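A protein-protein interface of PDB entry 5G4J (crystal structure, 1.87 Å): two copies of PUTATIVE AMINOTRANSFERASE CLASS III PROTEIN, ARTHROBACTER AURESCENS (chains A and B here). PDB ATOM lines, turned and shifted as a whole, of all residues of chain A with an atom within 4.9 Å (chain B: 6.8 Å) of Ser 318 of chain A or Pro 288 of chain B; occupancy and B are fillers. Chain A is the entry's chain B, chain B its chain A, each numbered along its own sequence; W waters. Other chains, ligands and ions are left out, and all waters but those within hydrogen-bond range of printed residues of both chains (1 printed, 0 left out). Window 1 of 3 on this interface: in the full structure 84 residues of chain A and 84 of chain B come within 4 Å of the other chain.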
ATOM      1  N   ASN A 118      -7.083   5.270 -15.508  1.00  0.00           N
ATOM      2  CA  ASN A 118      -8.362   4.974 -14.851  1.00  0.00           C
ATOM      3  C   ASN A 118      -9.502   5.950 -15.142  1.00  0.00           C
ATOM      4  O   ASN A 118     -10.556   5.852 -14.548  1.00  0.00           O
ATOM      5  CB  ASN A 118      -8.144   4.856 -13.345  1.00  0.00           C
ATOM      6  CG  ASN A 118      -6.958   3.991 -12.964  1.00  0.00           C
ATOM      7  OD1 ASN A 118      -5.862   4.506 -12.557  1.00  0.00           O
ATOM      8  ND2 ASN A 118      -7.072   2.737 -13.210  1.00  0.00           N
ATOM      9  N   HIS A 287     -16.767   0.786 -15.697  1.00  0.00           N
ATOM     10  CA  HIS A 287     -15.583   0.503 -14.981  1.00  0.00           C
ATOM     11  C   HIS A 287     -14.620   1.664 -15.176  1.00  0.00           C
ATOM     12  O   HIS A 287     -14.518   2.203 -16.256  1.00  0.00           O
ATOM     13  CB  HIS A 287     -14.973  -0.788 -15.467  1.00  0.00           C
ATOM     14  CG  HIS A 287     -14.102  -1.439 -14.466  1.00  0.00           C
ATOM     15  ND1 HIS A 287     -12.722  -1.289 -14.472  1.00  0.00           N
ATOM     16  CD2 HIS A 287     -14.391  -2.143 -13.373  1.00  0.00           C
ATOM     17  CE1 HIS A 287     -12.211  -1.965 -13.458  1.00  0.00           C
ATOM     18  NE2 HIS A 287     -13.196  -2.484 -12.784  1.00  0.00           N
ATOM     19  N   PRO A 288     -13.878   2.066 -14.140  1.00  0.00           N
ATOM     20  CA  PRO A 288     -12.986   3.224 -14.340  1.00  0.00           C
ATOM     21  C   PRO A 288     -11.776   2.846 -15.177  1.00  0.00           C
ATOM     22  O   PRO A 288     -10.879   2.149 -14.710  1.00  0.00           O
ATOM     23  CB  PRO A 288     -12.575   3.664 -12.898  1.00  0.00           C
ATOM     24  CG  PRO A 288     -13.453   2.877 -12.006  1.00  0.00           C
ATOM     25  CD  PRO A 288     -13.832   1.607 -12.752  1.00  0.00           C
ATOM     26  N   ILE A 289     -11.820   3.255 -16.458  1.00  0.00           N
ATOM     27  CA  ILE A 289     -10.694   2.965 -17.375  1.00  0.00           C
ATOM     28  C   ILE A 289     -10.608   4.144 -18.327  1.00  0.00           C
ATOM     29  O   ILE A 289     -11.668   4.748 -18.781  1.00  0.00           O
ATOM     30  CB  ILE A 289     -10.953   1.700 -18.239  1.00  0.00           C
ATOM     31  CG1 ILE A 289     -11.445   0.506 -17.455  1.00  0.00           C
ATOM     32  CG2 ILE A 289      -9.691   1.292 -19.045  1.00  0.00           C
ATOM     33  CD1 ILE A 289     -11.861  -0.697 -18.339  1.00  0.00           C
ATOM     34  N   PHE A 312      -3.330   1.267 -10.582  1.00  0.00           N
ATOM     35  CA  PHE A 312      -4.548   0.494 -10.992  1.00  0.00           C
ATOM     36  C   PHE A 312      -4.617   0.251 -12.494  1.00  0.00           C
ATOM     37  O   PHE A 312      -5.365  -0.690 -12.966  1.00  0.00           O
ATOM     38  CB  PHE A 312      -5.807   1.234 -10.610  1.00  0.00           C
ATOM     39  CG  PHE A 312      -5.967   1.400  -9.087  1.00  0.00           C
ATOM     40  CD1 PHE A 312      -5.702   0.315  -8.204  1.00  0.00           C
ATOM     41  CD2 PHE A 312      -6.361   2.640  -8.540  1.00  0.00           C
ATOM     42  CE1 PHE A 312      -5.864   0.448  -6.791  1.00  0.00           C
ATOM     43  CE2 PHE A 312      -6.519   2.746  -7.148  1.00  0.00           C
ATOM     44  CZ  PHE A 312      -6.311   1.638  -6.268  1.00  0.00           C
ATOM     45  N   ASN A 315      -4.782  -3.271 -14.638  1.00  0.00           N
ATOM     46  CA  ASN A 315      -4.931  -4.399 -13.759  1.00  0.00           C
ATOM     47  C   ASN A 315      -5.778  -5.386 -14.543  1.00  0.00           C
ATOM     48  O   ASN A 315      -6.454  -5.010 -15.454  1.00  0.00           O
ATOM     49  CB  ASN A 315      -5.577  -3.979 -12.416  1.00  0.00           C
ATOM     50  CG  ASN A 315      -7.038  -3.518 -12.550  1.00  0.00           C
ATOM     51  OD1 ASN A 315      -7.923  -4.329 -12.739  1.00  0.00           O
ATOM     52  ND2 ASN A 315      -7.286  -2.242 -12.439  1.00  0.00           N
ATOM     53  N   PRO A 316      -5.705  -6.640 -14.191  1.00  0.00           N
ATOM     54  CA  PRO A 316      -6.434  -7.660 -14.906  1.00  0.00           C
ATOM     55  C   PRO A 316      -7.945  -7.466 -14.959  1.00  0.00           C
ATOM     56  O   PRO A 316      -8.551  -7.820 -15.994  1.00  0.00           O
ATOM     57  CB  PRO A 316      -6.083  -8.931 -14.154  1.00  0.00           C
ATOM     58  CG  PRO A 316      -4.840  -8.628 -13.424  1.00  0.00           C
ATOM     59  CD  PRO A 316      -4.799  -7.179 -13.156  1.00  0.00           C
ATOM     60  N   VAL A 317      -8.550  -6.933 -13.881  1.00  0.00           N
ATOM     61  CA  VAL A 317     -10.023  -6.751 -13.861  1.00  0.00           C
ATOM     62  C   VAL A 317     -10.446  -5.684 -14.835  1.00  0.00           C
ATOM     63  O   VAL A 317     -11.404  -5.867 -15.581  1.00  0.00           O
ATOM     64  CB  VAL A 317     -10.533  -6.566 -12.422  1.00  0.00           C
ATOM     65  CG1 VAL A 317     -12.018  -6.252 -12.395  1.00  0.00           C
ATOM     66  CG2 VAL A 317     -10.286  -7.871 -11.659  1.00  0.00           C
ATOM     67  N   SER A 318      -9.770  -4.536 -14.850  1.00  0.00           N
ATOM     68  CA  SER A 318     -10.060  -3.481 -15.761  1.00  0.00           C
ATOM     69  C   SER A 318      -9.872  -3.942 -17.219  1.00  0.00           C
ATOM     70  O   SER A 318     -10.674  -3.614 -18.079  1.00  0.00           O
ATOM     71  CB  SER A 318      -9.204  -2.237 -15.529  1.00  0.00           C
ATOM     72  OG  SER A 318      -9.464  -1.624 -14.276  1.00  0.00           O
ATOM     73  N   SER A 319      -8.821  -4.718 -17.459  1.00  0.00           N
ATOM     74  CA  SER A 319      -8.576  -5.253 -18.783  1.00  0.00           C
ATOM     75  C   SER A 319      -9.677  -6.254 -19.191  1.00  0.00           C
ATOM     76  O   SER A 319     -10.109  -6.258 -20.341  1.00  0.00           O
ATOM     77  CB  SER A 319      -7.211  -5.964 -18.789  1.00  0.00           C
ATOM     78  OG  SER A 319      -6.206  -5.053 -18.391  1.00  0.00           O
ATOM     79  N   ALA A 320     -10.117  -7.063 -18.249  1.00  0.00           N
ATOM     80  CA  ALA A 320     -11.248  -7.973 -18.497  1.00  0.00           C
ATOM     81  C   ALA A 320     -12.495  -7.199 -18.908  1.00  0.00           C
ATOM     82  O   ALA A 320     -13.278  -7.588 -19.864  1.00  0.00           O
ATOM     83  CB  ALA A 320     -11.505  -8.848 -17.279  1.00  0.00           C
ATOM     84  N   ALA A 321     -12.745  -6.090 -18.228  1.00  0.00           N
ATOM     85  CA  ALA A 321     -13.935  -5.258 -18.528  1.00  0.00           C
ATOM     86  C   ALA A 321     -13.870  -4.693 -19.914  1.00  0.00           C
ATOM     87  O   ALA A 321     -14.866  -4.686 -20.700  1.00  0.00           O
ATOM     88  CB  ALA A 321     -14.085  -4.128 -17.531  1.00  0.00           C
ATOM     89  N   GLY A 322     -12.711  -4.140 -20.220  1.00  0.00           N
ATOM     90  CA  GLY A 322     -12.517  -3.524 -21.533  1.00  0.00           C
ATOM     91  C   GLY A 322     -12.613  -4.553 -22.665  1.00  0.00           C
ATOM     92  O   GLY A 322     -13.133  -4.257 -23.727  1.00  0.00           O
ATOM     93  N   THR B 117     -12.422   9.676  -6.075  1.00  0.00           N
ATOM     94  CA  THR B 117     -11.685   9.688  -7.331  1.00  0.00           C
ATOM     95  C   THR B 117     -11.461   8.262  -7.792  1.00  0.00           C
ATOM     96  O   THR B 117     -11.987   7.331  -7.185  1.00  0.00           O
ATOM     97  CB  THR B 117     -10.272  10.367  -7.178  1.00  0.00           C
ATOM     98  OG1 THR B 117      -9.426   9.546  -6.380  1.00  0.00           O
ATOM     99  CG2 THR B 117     -10.357  11.718  -6.551  1.00  0.00           C
ATOM    100  N   ASN B 118     -10.655   8.081  -8.846  1.00  0.00           N
ATOM    101  CA  ASN B 118     -10.362   6.703  -9.346  1.00  0.00           C
ATOM    102  C   ASN B 118      -8.933   6.220  -9.109  1.00  0.00           C
ATOM    103  O   ASN B 118      -8.571   5.162  -9.552  1.00  0.00           O
ATOM    104  CB  ASN B 118     -10.726   6.631 -10.824  1.00  0.00           C
ATOM    105  CG  ASN B 118     -12.072   7.228 -11.127  1.00  0.00           C
ATOM    106  OD1 ASN B 118     -12.192   8.320 -11.763  1.00  0.00           O
ATOM    107  ND2 ASN B 118     -13.077   6.543 -10.729  1.00  0.00           N
ATOM    108  N   SER B 119      -8.101   7.019  -8.414  1.00  0.00           N
ATOM    109  CA  SER B 119      -6.724   6.632  -8.129  1.00  0.00           C
ATOM    110  C   SER B 119      -6.151   7.557  -7.068  1.00  0.00           C
ATOM    111  O   SER B 119      -6.669   8.665  -6.802  1.00  0.00           O
ATOM    112  CB  SER B 119      -5.833   6.777  -9.384  1.00  0.00           C
ATOM    113  OG  SER B 119      -5.730   8.143  -9.797  1.00  0.00           O
ATOM    114  N   MET B 283      -8.006   0.631  -1.080  1.00  0.00           N
ATOM    115  CA  MET B 283      -9.369   0.904  -0.692  1.00  0.00           C
ATOM    116  C   MET B 283     -10.479   0.062  -1.340  1.00  0.00           C
ATOM    117  O   MET B 283     -11.559  -0.196  -0.738  1.00  0.00           O
ATOM    118  CB  MET B 283      -9.587   2.409  -0.696  1.00  0.00           C
ATOM    119  CG  MET B 283     -10.165   3.056  -1.818  1.00  0.00           C
ATOM    120  SD  MET B 283     -10.055   4.902  -1.636  1.00  0.00           S
ATOM    121  CE  MET B 283     -11.668   5.357  -1.076  1.00  0.00           C
ATOM    122  N   GLY B 284     -10.279  -0.345  -2.616  1.00  0.00           N
ATOM    123  CA  GLY B 284     -11.204  -1.223  -3.323  1.00  0.00           C
ATOM    124  C   GLY B 284     -10.665  -2.623  -3.582  1.00  0.00           C
ATOM    125  O   GLY B 284     -11.121  -3.310  -4.485  1.00  0.00           O
ATOM    126  N   GLY B 286      -8.120  -3.434  -5.153  1.00  0.00           N
ATOM    127  CA  GLY B 286      -7.747  -3.545  -6.594  1.00  0.00           C
ATOM    128  C   GLY B 286      -8.589  -2.812  -7.577  1.00  0.00           C
ATOM    129  O   GLY B 286      -8.106  -2.450  -8.659  1.00  0.00           O
ATOM    130  N   HIS B 287      -9.801  -2.525  -7.153  1.00  0.00           N
ATOM    131  CA  HIS B 287     -10.689  -1.658  -7.917  1.00  0.00           C
ATOM    132  C   HIS B 287     -10.133  -0.255  -7.964  1.00  0.00           C
ATOM    133  O   HIS B 287      -9.626   0.211  -6.987  1.00  0.00           O
ATOM    134  CB  HIS B 287     -12.083  -1.661  -7.313  1.00  0.00           C
ATOM    135  CG  HIS B 287     -13.162  -1.321  -8.294  1.00  0.00           C
ATOM    136  ND1 HIS B 287     -13.732  -0.079  -8.396  1.00  0.00           N
ATOM    137  CD2 HIS B 287     -13.777  -2.082  -9.208  1.00  0.00           C
ATOM    138  CE1 HIS B 287     -14.620  -0.076  -9.356  1.00  0.00           C
ATOM    139  NE2 HIS B 287     -14.665  -1.289  -9.864  1.00  0.00           N
ATOM    140  N   PRO B 288     -10.193   0.433  -9.122  1.00  0.00           N
ATOM    141  CA  PRO B 288      -9.647   1.817  -9.175  1.00  0.00           C
ATOM    142  C   PRO B 288     -10.491   2.813  -8.403  1.00  0.00           C
ATOM    143  O   PRO B 288     -11.596   3.152  -8.819  1.00  0.00           O
ATOM    144  CB  PRO B 288      -9.617   2.128 -10.667  1.00  0.00           C
ATOM    145  CG  PRO B 288      -9.978   0.812 -11.371  1.00  0.00           C
ATOM    146  CD  PRO B 288     -10.801   0.018 -10.405  1.00  0.00           C
ATOM    147  N   ILE B 289     -10.074   3.138  -7.179  1.00  0.00           N
ATOM    148  CA  ILE B 289     -10.811   4.097  -6.360  1.00  0.00           C
ATOM    149  C   ILE B 289      -9.666   4.875  -5.622  1.00  0.00           C
ATOM    150  O   ILE B 289      -8.636   4.278  -5.173  1.00  0.00           O
ATOM    151  CB  ILE B 289     -11.668   3.411  -5.275  1.00  0.00           C
ATOM    152  CG1 ILE B 289     -12.525   2.265  -5.807  1.00  0.00           C
ATOM    153  CG2 ILE B 289     -12.551   4.409  -4.550  1.00  0.00           C
ATOM    154  CD1 ILE B 289     -13.290   1.471  -4.717  1.00  0.00           C
ATOM    155  N   GLY B 290      -9.914   6.157  -5.439  1.00  0.00           N
ATOM    156  CA  GLY B 290      -9.201   6.980  -4.486  1.00  0.00           C
ATOM    157  C   GLY B 290     -10.160   7.918  -3.797  1.00  0.00           C
ATOM    158  O   GLY B 290     -11.368   7.951  -4.089  1.00  0.00           O
ATOM    159  N   PHE B 312     -16.436   8.712 -13.334  1.00  0.00           N
ATOM    160  CA  PHE B 312     -16.470   7.341 -12.731  1.00  0.00           C
ATOM    161  C   PHE B 312     -16.492   7.378 -11.207  1.00  0.00           C
ATOM    162  O   PHE B 312     -16.926   6.408 -10.556  1.00  0.00           O
ATOM    163  CB  PHE B 312     -15.224   6.562 -13.166  1.00  0.00           C
ATOM    164  CG  PHE B 312     -15.152   6.316 -14.646  1.00  0.00           C
ATOM    165  CD1 PHE B 312     -16.288   5.901 -15.355  1.00  0.00           C
ATOM    166  CD2 PHE B 312     -13.947   6.439 -15.326  1.00  0.00           C
ATOM    167  CE1 PHE B 312     -16.229   5.568 -16.745  1.00  0.00           C
ATOM    168  CE2 PHE B 312     -13.922   6.138 -16.738  1.00  0.00           C
ATOM    169  CZ  PHE B 312     -15.070   5.710 -17.411  1.00  0.00           C
ATOM    170  N   ASN B 315     -19.262   5.979  -8.556  1.00  0.00           N
ATOM    171  CA  ASN B 315     -20.254   5.123  -9.179  1.00  0.00           C
ATOM    172  C   ASN B 315     -20.628   4.013  -8.217  1.00  0.00           C
ATOM    173  O   ASN B 315     -19.874   3.701  -7.320  1.00  0.00           O
ATOM    174  CB  ASN B 315     -19.713   4.564 -10.504  1.00  0.00           C
ATOM    175  CG  ASN B 315     -18.575   3.529 -10.321  1.00  0.00           C
ATOM    176  OD1 ASN B 315     -18.838   2.368 -10.002  1.00  0.00           O
ATOM    177  ND2 ASN B 315     -17.361   3.927 -10.582  1.00  0.00           N
ATOM    178  N   SER B 318     -17.925   0.957  -7.758  1.00  0.00           N
ATOM    179  CA  SER B 318     -16.783   1.354  -6.966  1.00  0.00           C
ATOM    180  C   SER B 318     -17.137   1.461  -5.472  1.00  0.00           C
ATOM    181  O   SER B 318     -16.387   1.052  -4.620  1.00  0.00           O
ATOM    182  CB  SER B 318     -16.186   2.687  -7.457  1.00  0.00           C
ATOM    183  OG  SER B 318     -15.618   2.556  -8.761  1.00  0.00           O
HETATM  184  O   HOH W   1     -10.098  -3.482 -10.996  1.00  0.00           O
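Among the printed residues, merely in contact across the chains: Asn 118 of chain A with Asn 118 of chain B (3.8 Å), Asn 118 of chain A with Ser 119 of chain B (3.9 Å), Asn 118 of chain A with Pro 288 of chain B (3.6 Å), Asn 118 of chain A with Phe 312 of chain B (3.5 Å), His 287 of chain A with Pro 288 of chain B (3.9 Å), His 287 of chain A with Phe 312 of chain B (3.7 Å), Pro 288 of chain A with Asn 118 of chain B (3.6 Å), Pro 288 of chain A with His 287 of chain B (3.9 Å), Pro 288 of chain A with Pro 288 of chain B (3.7 Å), Pro 288 of chain A with Phe 312 of chain B (3.5 Å), Pro 288 of chain A with Ser 318 of chain B (3.9 Å), Ile 289 of chain A with Phe 312 of chain B (3.3 Å), Phe 312 of chain A with Asn 118 of chain B (3.5 Å), Phe 312 of chain A with Gly 286 of chain B (3.7 Å), Phe 312 of chain A with His 287 of chain B (3.7 Å), Phe 312 of chain A with Pro 288 of chain B (3.4 Å), Phe 312 of chain A with Ile 289 of chain B (3.3 Å), Asn 315 of chain A with Gly 286 of chain B (3.9 Å) and Ser 318 of chain A with Pro 288 of chain B (3.8 Å).
A ring nitrogen (NE2) of His 287 of chain B sits at hydrogen-bond distance from a ring nitrogen (NE2) of His 287 of chain A (3.5 Å).
Val 317 of chain A touches none of the printed residues of chain B. Of chain B, only Pro 288 (3.8 Å) comes within 4 Å of Ser 318 of chain A. Ala 321 of chain A touches none of the printed residues of chain B. Of the printed residues of chain A, His 287 of chain B touches His 287, Pro 288 and Phe 312. Of the printed residues of chain A, Ile 289 of chain B touches Phe 312 (3.3 Å). The nearest residue of chain A that does not touch Pro 288 of chain B is Asn 315 of chain A (4.2 Å). The nearest printed residue of chain A that does not touch His 287 of chain B is Val 317 of chain A (5.5 Å).
Asn 118 of chain B touches its own counterpart, Asn 118 of chain A. His 287 of chain B touches its own counterpart, His 287 of chain A. His 287 of chain A touches Pro 288 of chain B, and with the chains exchanged Pro 288 of chain A touches His 287 of chain B. Pro 288 of chain B touches its own counterpart, Pro 288 of chain A. Positions printed for both chains: 118, 287, 288, 289, 312, 315 and 318.
Water W1 lies within hydrogen-bond range of the side-chain amide oxygen of Asn 315 of chain A (2.9 Å) and the backbone carbonyl oxygen of Gly 286 of chain B (3.2 Å).
Hydrophobic or aromatic side chains of chain B that line the printed part of chain A: His 287, Pro 288 and Phe 312. Of the 13 printed residues of chain A, 7 touch a printed residue of chain B. Hydrophobic or aromatic side chains of chain A within 4 Å of the printed part of chain B: His 287, Pro 288 and Phe 312.
ND1 of His 287 of chain A lies close to OG of Ser 318 of chain A, at 3.3 Å. O of Asn 315 of chain A is in hydrogen-bond range of OG of Ser 319 of chain A (2.9 Å). The backbone carbonyl oxygen of Phe 312 of chain A is in hydrogen-bond range of the side-chain amide nitrogen of Asn 315 of chain A, at 2.5 Å. The backbone carbonyl oxygen (O) of Asn 118 of chain A is in hydrogen-bond range of the backbone NH (N) of Ile 289 of chain A, at 3.5 Å. N of Ile 289 of chain B lies within hydrogen-bond range of O of Asn 118 of chain B, at 3.5 Å. The side-chain amide oxygen of Asn 315 of chain A sits at hydrogen-bond distance from the backbone NH of Val 317 of chain A (2.9 Å).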
